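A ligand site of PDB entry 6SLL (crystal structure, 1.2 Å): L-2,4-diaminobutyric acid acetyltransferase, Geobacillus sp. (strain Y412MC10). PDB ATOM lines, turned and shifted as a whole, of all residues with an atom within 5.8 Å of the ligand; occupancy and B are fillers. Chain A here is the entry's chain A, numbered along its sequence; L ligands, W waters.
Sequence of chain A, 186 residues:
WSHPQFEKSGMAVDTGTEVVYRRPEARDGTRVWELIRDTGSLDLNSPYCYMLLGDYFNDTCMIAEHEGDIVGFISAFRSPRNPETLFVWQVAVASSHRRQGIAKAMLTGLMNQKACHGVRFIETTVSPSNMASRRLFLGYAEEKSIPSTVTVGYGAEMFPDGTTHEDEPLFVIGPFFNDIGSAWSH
Water W9 bridges an oxygen (O3) of the ligand and the backbone carbonyl oxygen (O) of Arg 135.
Water W8 lies within hydrogen-bond range of the backbone carbonyl oxygen (O) of Val 91 (2.7 Å) and an oxygen (O16) of the ligand (2.7 Å).
Water W6 bridges an oxygen (O1) of the ligand (2.8 Å) and the guanidinium group (NE) of Arg 99 (3.1 Å).
Water W2 lies within hydrogen-bond range of O16 of the ligand (3.1 Å) and ND2 of Asn 130 (3.1 Å).
Merely in contact with the ligand: Leu 42, Val 91, Ala 92, Arg 98, Ile 102, Ala 132, Ser 133 and Leu 136.
Within 4 Å of the ligand: Ser 41, Leu 42, Val 91, Ala 92, Val 93, Arg 98, Arg 99, Gln 100, Gly 101, Ile 102, Ala 103, Lys 104, Asn 130, Ala 132, Ser 133, Arg 135 and Leu 136.
The backbone carbonyl oxygen (O) of Ser 41 sits close to a nitrogen (N7) of the ligand, at 3.4 Å.
A nitrogen (N7) of the ligand sits at hydrogen-bond distance from the side-chain hydroxyl (OG) of Ser 41.
The backbone NH (N) of Arg 99 sits at hydrogen-bond distance from an oxygen (O11) of the ligand, at 2.8 Å.
O15 of the ligand is in hydrogen-bond range of N of Val 93, 2.9 Å away.
N of Gly 101 sits at hydrogen-bond distance from O9 of the ligand (2.9 Å).
The side-chain amide nitrogen of Asn 130 lies within hydrogen-bond range of an oxygen (O16) of the ligand (2.9 Å).
N of Lys 104 is in hydrogen-bond range of O8 of the ligand.
O3 of the ligand is in salt-bridge range of NZ of Lys 104, at 3.2 Å.
N of Ala 103 sits at hydrogen-bond distance from O12 of the ligand (3.0 Å).
The guanidinium group (NE) of Arg 135 is in salt-bridge range of an oxygen (O4) of the ligand.
The backbone NH (N) of Gln 100 is in hydrogen-bond range of an oxygen (O9) of the ligand, at 3.5 Å.
The backbone NH (N) of Ser 41 lies close to the side-chain hydroxyl (OG1) of Thr 39, at 3.3 Å.
NE of Arg 98 is in hydrogen-bond range of O of Val 93 (2.8 Å).
The side-chain amide oxygen (OD1) of Asn 130 sits at hydrogen-bond distance from the backbone NH (N) of Ser 133 (3.0 Å).
N of Leu 42 sits at hydrogen-bond distance from OG1 of Thr 39.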
ATOM      1  N   THR A  39      -9.616  10.534  17.549  1.00  0.00           N
ATOM      2  CA  THR A  39      -9.257  11.309  18.714  1.00  0.00           C
ATOM      3  C   THR A  39      -7.752  11.352  18.899  1.00  0.00           C
ATOM      4  O   THR A  39      -7.238  12.319  19.496  1.00  0.00           O
ATOM      5  CB  THR A  39      -9.883  10.895  20.066  1.00  0.00           C
ATOM      6  OG1 THR A  39      -9.360   9.646  20.505  1.00  0.00           O
ATOM      7  CG2 THR A  39     -11.483  10.843  19.939  1.00  0.00           C
ATOM      8  N   SER A  41      -6.111   9.972  21.058  1.00  0.00           N
ATOM      9  CA  SER A  41      -5.842  10.086  22.477  1.00  0.00           C
ATOM     10  C   SER A  41      -6.570   9.055  23.390  1.00  0.00           C
ATOM     11  O   SER A  41      -6.575   9.260  24.588  1.00  0.00           O
ATOM     12  CB  SER A  41      -6.116  11.486  22.944  1.00  0.00           C
ATOM     13  OG  SER A  41      -7.501  11.770  22.763  1.00  0.00           O
ATOM     14  N   LEU A  42      -7.333   8.185  22.928  1.00  0.00           N
ATOM     15  CA  LEU A  42      -7.957   7.073  23.632  1.00  0.00           C
ATOM     16  C   LEU A  42      -7.203   5.883  23.210  1.00  0.00           C
ATOM     17  O   LEU A  42      -6.647   5.752  22.145  1.00  0.00           O
ATOM     18  CB  LEU A  42      -9.420   7.026  23.319  1.00  0.00           C
ATOM     19  CG  LEU A  42     -10.318   8.049  23.847  1.00  0.00           C
ATOM     20  CD1 LEU A  42     -11.690   8.073  23.217  1.00  0.00           C
ATOM     21  CD2 LEU A  42     -10.541   7.859  25.350  1.00  0.00           C
ATOM     22  N   VAL A  91     -15.337   7.508  26.618  1.00  0.00           N
ATOM     23  CA  VAL A  91     -16.168   8.619  26.207  1.00  0.00           C
ATOM     24  C   VAL A  91     -15.418   9.432  25.163  1.00  0.00           C
ATOM     25  O   VAL A  91     -14.264   9.820  25.414  1.00  0.00           O
ATOM     26  CB  VAL A  91     -16.565   9.553  27.379  1.00  0.00           C
ATOM     27  CG1 VAL A  91     -17.530  10.620  26.903  1.00  0.00           C
ATOM     28  CG2 VAL A  91     -17.091   8.809  28.576  1.00  0.00           C
ATOM     29  N   ALA A  92     -16.022   9.611  23.989  1.00  0.00           N
ATOM     30  CA  ALA A  92     -15.346  10.336  22.904  1.00  0.00           C
ATOM     31  C   ALA A  92     -16.290  11.283  22.266  1.00  0.00           C
ATOM     32  O   ALA A  92     -17.457  10.875  21.960  1.00  0.00           O
ATOM     33  CB  ALA A  92     -14.838   9.380  21.877  1.00  0.00           C
ATOM     34  N   VAL A  93     -15.864  12.507  21.974  1.00  0.00           N
ATOM     35  CA  VAL A  93     -16.598  13.483  21.165  1.00  0.00           C
ATOM     36  C   VAL A  93     -15.676  14.004  20.131  1.00  0.00           C
ATOM     37  O   VAL A  93     -14.478  14.315  20.408  1.00  0.00           O
ATOM     38  CB  VAL A  93     -17.201  14.612  22.040  1.00  0.00           C
ATOM     39  CG1 VAL A  93     -17.784  15.709  21.185  1.00  0.00           C
ATOM     40  CG2 VAL A  93     -18.254  14.069  22.957  1.00  0.00           C
ATOM     41  N   ALA A  94     -16.112  13.961  18.873  1.00  0.00           N
ATOM     42  CA  ALA A  94     -15.270  14.469  17.720  1.00  0.00           C
ATOM     43  C   ALA A  94     -14.837  15.918  18.015  1.00  0.00           C
ATOM     44  O   ALA A  94     -15.577  16.743  18.536  1.00  0.00           O
ATOM     45  CB  ALA A  94     -16.030  14.469  16.470  1.00  0.00           C
ATOM     46  N   HIS A  97     -17.026  18.964  17.426  1.00  0.00           N
ATOM     47  CA  HIS A  97     -18.229  19.061  18.192  1.00  0.00           C
ATOM     48  C   HIS A  97     -18.029  19.136  19.689  1.00  0.00           C
ATOM     49  O   HIS A  97     -18.958  19.088  20.463  1.00  0.00           O
ATOM     50  CB  HIS A  97     -19.098  17.947  17.837  1.00  0.00           C
ATOM     51  CG  HIS A  97     -19.762  18.058  16.517  1.00  0.00           C
ATOM     52  ND1 HIS A  97     -19.140  17.860  15.315  1.00  0.00           N
ATOM     53  CD2 HIS A  97     -21.051  18.382  16.175  1.00  0.00           C
ATOM     54  CE1 HIS A  97     -19.974  18.085  14.265  1.00  0.00           C
ATOM     55  NE2 HIS A  97     -21.145  18.383  14.801  1.00  0.00           N
ATOM     56  N   ARG A  98     -16.769  19.445  20.123  1.00  0.00           N
ATOM     57  CA  ARG A  98     -16.479  19.532  21.525  1.00  0.00           C
ATOM     58  C   ARG A  98     -16.927  20.824  22.195  1.00  0.00           C
ATOM     59  O   ARG A  98     -17.143  21.858  21.457  1.00  0.00           O
ATOM     60  CB  ARG A  98     -14.984  19.283  21.821  1.00  0.00           C
ATOM     61  CG  ARG A  98     -14.557  17.828  21.634  1.00  0.00           C
ATOM     62  CD  ARG A  98     -13.061  17.623  21.818  1.00  0.00           C
ATOM     63  NE  ARG A  98     -12.734  16.301  21.394  1.00  0.00           N
ATOM     64  CZ  ARG A  98     -11.555  15.953  20.930  1.00  0.00           C
ATOM     65  NH1 ARG A  98     -10.476  16.768  21.096  1.00  0.00           N
ATOM     66  NH2 ARG A  98     -11.429  14.852  20.275  1.00  0.00           N
ATOM     67  N   ARG A  99     -17.162  20.804  23.468  1.00  0.00           N
ATOM     68  CA  ARG A  99     -17.534  21.946  24.260  1.00  0.00           C
ATOM     69  C   ARG A  99     -18.878  22.506  23.902  1.00  0.00           C
ATOM     70  O   ARG A  99     -19.176  23.700  24.024  1.00  0.00           O
ATOM     71  CB  ARG A  99     -16.449  23.058  24.278  1.00  0.00           C
ATOM     72  CG  ARG A  99     -15.071  22.572  24.477  1.00  0.00           C
ATOM     73  CD  ARG A  99     -14.101  23.660  24.752  1.00  0.00           C
ATOM     74  NE  ARG A  99     -14.366  24.226  26.099  1.00  0.00           N
ATOM     75  CZ  ARG A  99     -13.629  25.176  26.607  1.00  0.00           C
ATOM     76  NH1 ARG A  99     -12.534  25.717  25.983  1.00  0.00           N
ATOM     77  NH2 ARG A  99     -13.960  25.591  27.803  1.00  0.00           N
ATOM     78  N   GLN A 100     -19.788  21.608  23.524  1.00  0.00           N
ATOM     79  CA  GLN A 100     -21.191  21.867  23.247  1.00  0.00           C
ATOM     80  C   GLN A 100     -22.160  21.109  24.206  1.00  0.00           C
ATOM     81  O   GLN A 100     -23.355  21.090  23.955  1.00  0.00           O
ATOM     82  CB  GLN A 100     -21.552  21.467  21.744  1.00  0.00           C
ATOM     83  CG  GLN A 100     -20.763  22.120  20.691  1.00  0.00           C
ATOM     84  CD  GLN A 100     -21.291  21.627  19.276  1.00  0.00           C
ATOM     85  OE1 GLN A 100     -22.436  20.914  19.131  1.00  0.00           O
ATOM     86  NE2 GLN A 100     -20.476  21.844  18.309  1.00  0.00           N
ATOM     87  N   GLY A 101     -21.595  20.357  25.145  1.00  0.00           N
ATOM     88  CA  GLY A 101     -22.397  19.645  26.081  1.00  0.00           C
ATOM     89  C   GLY A 101     -22.797  18.197  25.567  1.00  0.00           C
ATOM     90  O   GLY A 101     -23.592  17.605  26.231  1.00  0.00           O
ATOM     91  N   ILE A 102     -22.125  17.777  24.509  1.00  0.00           N
ATOM     92  CA  ILE A 102     -22.534  16.423  24.001  1.00  0.00           C
ATOM     93  C   ILE A 102     -22.141  15.333  24.967  1.00  0.00           C
ATOM     94  O   ILE A 102     -22.922  14.414  25.240  1.00  0.00           O
ATOM     95  CB  ILE A 102     -21.981  16.208  22.611  1.00  0.00           C
ATOM     96  CG1 ILE A 102     -22.594  17.166  21.621  1.00  0.00           C
ATOM     97  CG2 ILE A 102     -22.191  14.781  22.158  1.00  0.00           C
ATOM     98  CD1 ILE A 102     -21.931  17.168  20.296  1.00  0.00           C
ATOM     99  N   ALA A 103     -20.911  15.380  25.546  1.00  0.00           N
ATOM    100  CA  ALA A 103     -20.563  14.375  26.520  1.00  0.00           C
ATOM    101  C   ALA A 103     -21.476  14.365  27.731  1.00  0.00           C
ATOM    102  O   ALA A 103     -21.921  13.313  28.190  1.00  0.00           O
ATOM    103  CB  ALA A 103     -19.081  14.466  26.936  1.00  0.00           C
ATOM    104  N   LYS A 104     -21.793  15.567  28.237  1.00  0.00           N
ATOM    105  CA  LYS A 104     -22.748  15.645  29.396  1.00  0.00           C
ATOM    106  C   LYS A 104     -24.078  15.075  29.027  1.00  0.00           C
ATOM    107  O   LYS A 104     -24.710  14.388  29.856  1.00  0.00           O
ATOM    108  CB  LYS A 104     -22.892  17.133  29.923  1.00  0.00           C
ATOM    109  CG  LYS A 104     -21.608  17.597  30.505  1.00  0.00           C
ATOM    110  CD  LYS A 104     -21.623  19.092  30.870  1.00  0.00           C
ATOM    111  CE  LYS A 104     -22.641  19.291  31.897  1.00  0.00           C
ATOM    112  NZ  LYS A 104     -22.423  20.619  32.487  1.00  0.00           N
ATOM    113  N   ALA A 105     -24.558  15.376  27.805  1.00  0.00           N
ATOM    114  CA  ALA A 105     -25.850  14.897  27.368  1.00  0.00           C
ATOM    115  C   ALA A 105     -25.855  13.372  27.212  1.00  0.00           C
ATOM    116  O   ALA A 105     -26.791  12.672  27.600  1.00  0.00           O
ATOM    117  CB  ALA A 105     -26.329  15.519  26.100  1.00  0.00           C
ATOM    118  N   SER A 129      -3.732  14.034  32.796  1.00  0.00           N
ATOM    119  CA  SER A 129      -3.715  15.117  31.857  1.00  0.00           C
ATOM    120  C   SER A 129      -5.063  15.325  31.143  1.00  0.00           C
ATOM    121  O   SER A 129      -5.270  16.314  30.433  1.00  0.00           O
ATOM    122  CB  SER A 129      -2.545  14.869  30.853  1.00  0.00           C
ATOM    123  OG  SER A 129      -1.292  14.763  31.486  1.00  0.00           O
ATOM    124  N   ASN A 130      -6.049  14.425  31.417  1.00  0.00           N
ATOM    125  CA  ASN A 130      -7.323  14.535  30.776  1.00  0.00           C
ATOM    126  C   ASN A 130      -8.284  15.406  31.528  1.00  0.00           C
ATOM    127  O   ASN A 130      -9.231  14.968  32.174  1.00  0.00           O
ATOM    128  CB  ASN A 130      -7.841  13.237  30.542  1.00  0.00           C
ATOM    129  CG  ASN A 130      -8.942  13.299  29.658  1.00  0.00           C
ATOM    130  OD1 ASN A 130      -9.487  14.386  29.459  1.00  0.00           O
ATOM    131  ND2 ASN A 130      -9.231  12.210  29.098  1.00  0.00           N
ATOM    132  N   MET A 131      -8.018  16.671  31.362  1.00  0.00           N
ATOM    133  CA  MET A 131      -8.654  17.682  32.187  1.00  0.00           C
ATOM    134  C   MET A 131     -10.155  17.717  31.889  1.00  0.00           C
ATOM    135  O   MET A 131     -10.976  17.934  32.824  1.00  0.00           O
ATOM    136  CB  MET A 131      -7.984  19.046  32.001  1.00  0.00           C
ATOM    137  CG  MET A 131      -6.552  19.018  32.557  1.00  0.00           C
ATOM    138  SD  MET A 131      -5.585  20.425  32.181  1.00  0.00           S
ATOM    139  CE  MET A 131      -6.607  21.731  32.851  1.00  0.00           C
ATOM    140  N   ALA A 132     -10.524  17.627  30.633  1.00  0.00           N
ATOM    141  CA  ALA A 132     -11.934  17.684  30.243  1.00  0.00           C
ATOM    142  C   ALA A 132     -12.705  16.460  30.761  1.00  0.00           C
ATOM    143  O   ALA A 132     -13.839  16.625  31.246  1.00  0.00           O
ATOM    144  CB  ALA A 132     -12.093  17.814  28.770  1.00  0.00           C
ATOM    145  N   SER A 133     -12.114  15.309  30.686  1.00  0.00           N
ATOM    146  CA  SER A 133     -12.785  14.128  31.244  1.00  0.00           C
ATOM    147  C   SER A 133     -12.960  14.233  32.733  1.00  0.00           C
ATOM    148  O   SER A 133     -14.010  13.869  33.263  1.00  0.00           O
ATOM    149  CB  SER A 133     -11.994  12.922  30.910  1.00  0.00           C
ATOM    150  OG  SER A 133     -12.556  11.770  31.466  1.00  0.00           O
ATOM    151  N   ARG A 135     -13.394  16.980  34.419  1.00  0.00           N
ATOM    152  CA  ARG A 135     -14.486  17.903  34.578  1.00  0.00           C
ATOM    153  C   ARG A 135     -15.858  17.269  34.264  1.00  0.00           C
ATOM    154  O   ARG A 135     -16.848  17.536  34.961  1.00  0.00           O
ATOM    155  CB  ARG A 135     -14.261  19.160  33.825  1.00  0.00           C
ATOM    156  CG  ARG A 135     -13.255  20.076  34.309  1.00  0.00           C
ATOM    157  CD  ARG A 135     -13.458  20.467  35.735  1.00  0.00           C
ATOM    158  NE  ARG A 135     -14.842  20.812  36.044  1.00  0.00           N
ATOM    159  CZ  ARG A 135     -15.445  20.547  37.267  1.00  0.00           C
ATOM    160  NH1 ARG A 135     -14.757  20.002  38.269  1.00  0.00           N
ATOM    161  NH2 ARG A 135     -16.755  20.903  37.380  1.00  0.00           N
ATOM    162  N   LEU A 136     -15.895  16.437  33.230  1.00  0.00           N
ATOM    163  CA  LEU A 136     -17.156  15.750  32.904  1.00  0.00           C
ATOM    164  C   LEU A 136     -17.635  14.976  34.114  1.00  0.00           C
ATOM    165  O   LEU A 136     -18.799  15.089  34.546  1.00  0.00           O
ATOM    166  CB  LEU A 136     -16.926  14.811  31.786  1.00  0.00           C
ATOM    167  CG  LEU A 136     -18.106  13.893  31.380  1.00  0.00           C
ATOM    168  CD1 LEU A 136     -19.325  14.679  30.932  1.00  0.00           C
ATOM    169  CD2 LEU A 136     -17.648  12.915  30.333  1.00  0.00           C
ATOM    170  N   GLY A 139     -17.905  17.178  37.473  1.00  0.00           N
ATOM    171  CA  GLY A 139     -19.031  18.091  37.312  1.00  0.00           C
ATOM    172  C   GLY A 139     -20.367  17.357  37.427  1.00  0.00           C
ATOM    173  O   GLY A 139     -21.336  17.865  38.009  1.00  0.00           O
HETATM  174  N1  LIG L   1     -11.387  23.031  28.113  1.00  0.00           N
HETATM  175  C1  LIG L   1     -11.878  23.118  29.387  1.00  0.00           C
HETATM  176  N2  LIG L   1     -13.063  22.563  29.815  1.00  0.00           N
HETATM  177  C2  LIG L   1     -13.449  21.517  28.974  1.00  0.00           C
HETATM  178  C3  LIG L   1     -12.964  21.397  27.649  1.00  0.00           C
HETATM  179  C4  LIG L   1     -11.740  21.992  27.331  1.00  0.00           C
HETATM  180  N3  LIG L   1     -11.180  21.899  26.091  1.00  0.00           N
HETATM  181  N4  LIG L   1     -13.699  20.462  26.971  1.00  0.00           N
HETATM  182  C5  LIG L   1     -14.605  20.231  27.902  1.00  0.00           C
HETATM  183  N5  LIG L   1     -14.575  20.906  29.002  1.00  0.00           N
HETATM  184  C6  LIG L   1     -15.399  20.801  30.174  1.00  0.00           C
HETATM  185  C7  LIG L   1     -16.812  21.559  30.028  1.00  0.00           C
HETATM  186  O1  LIG L   1     -16.728  22.941  30.392  1.00  0.00           O
HETATM  187  C8  LIG L   1     -17.677  20.760  30.970  1.00  0.00           C
HETATM  188  O2  LIG L   1     -17.252  21.023  32.323  1.00  0.00           O
HETATM  189  P1  LIG L   1     -18.291  21.973  33.155  1.00  0.00           P
HETATM  190  O3  LIG L   1     -19.436  21.049  33.452  1.00  0.00           O
HETATM  191  O4  LIG L   1     -17.324  22.386  34.350  1.00  0.00           O
HETATM  192  O5  LIG L   1     -18.748  23.166  32.340  1.00  0.00           O
HETATM  193  C9  LIG L   1     -17.071  19.293  30.899  1.00  0.00           C
HETATM  194  O6  LIG L   1     -15.759  19.498  30.309  1.00  0.00           O
HETATM  195  C10 LIG L   1     -17.986  18.474  29.850  1.00  0.00           C
HETATM  196  O7  LIG L   1     -18.307  19.319  28.706  1.00  0.00           O
HETATM  197  P2  LIG L   1     -18.922  18.745  27.366  1.00  0.00           P
HETATM  198  O8  LIG L   1     -20.087  17.857  27.684  1.00  0.00           O
HETATM  199  O9  LIG L   1     -19.079  19.897  26.435  1.00  0.00           O
HETATM  200  O10 LIG L   1     -17.684  17.871  26.886  1.00  0.00           O
HETATM  201  P3  LIG L   1     -17.376  17.390  25.378  1.00  0.00           P
HETATM  202  O11 LIG L   1     -16.485  18.401  24.737  1.00  0.00           O
HETATM  203  O12 LIG L   1     -18.623  17.070  24.650  1.00  0.00           O
HETATM  204  O13 LIG L   1     -16.572  16.051  25.610  1.00  0.00           O
HETATM  205  C11 LIG L   1     -14.633  14.751  26.158  1.00  0.00           C
HETATM  206  C12 LIG L   1     -15.540  15.863  26.576  1.00  0.00           C
HETATM  207  C13 LIG L   1     -13.633  14.410  27.289  1.00  0.00           C
HETATM  208  C14 LIG L   1     -15.408  13.475  25.845  1.00  0.00           C
HETATM  209  C15 LIG L   1     -13.806  15.209  24.969  1.00  0.00           C
HETATM  210  O14 LIG L   1     -12.852  16.238  25.364  1.00  0.00           O
HETATM  211  C16 LIG L   1     -13.096  14.179  24.210  1.00  0.00           C
HETATM  212  O15 LIG L   1     -13.605  13.319  23.512  1.00  0.00           O
HETATM  213  N6  LIG L   1     -11.744  14.149  24.247  1.00  0.00           N
HETATM  214  C17 LIG L   1     -10.947  13.213  23.434  1.00  0.00           C
HETATM  215  C18 LIG L   1     -10.886  11.844  24.140  1.00  0.00           C
HETATM  216  C19 LIG L   1     -10.054  11.866  25.405  1.00  0.00           C
HETATM  217  O16 LIG L   1     -10.505  11.913  26.535  1.00  0.00           O
HETATM  218  N7  LIG L   1      -8.754  11.812  25.160  1.00  0.00           N
HETATM  219  C20 LIG L   1      -7.769  11.964  26.091  1.00  0.00           C
HETATM  220  C21 LIG L   1      -7.364  13.376  26.454  1.00  0.00           C
HETATM  221  S1  LIG L   1      -6.282  14.496  25.550  1.00  0.00           S
HETATM  222  O   HOH W   1     -12.034  20.443  23.728  1.00  0.00           O
HETATM  223  O   HOH W   2     -10.370   9.403  28.286  1.00  0.00           O
HETATM  224  O   HOH W   3     -19.806  18.812  23.015  1.00  0.00           O
HETATM  225  O   HOH W   4     -19.566  22.334  27.510  1.00  0.00           O
HETATM  226  O   HOH W   5     -13.863  18.741  25.081  1.00  0.00           O
HETATM  227  O   HOH W   6     -16.912  23.916  27.798  1.00  0.00           O
HETATM  228  O   HOH W   7      -9.589  16.386  24.999  1.00  0.00           O
HETATM  229  O   HOH W   8     -12.722  10.596  27.487  1.00  0.00           O
HETATM  230  O   HOH W   9     -19.139  18.582  33.589  1.00  0.00           O
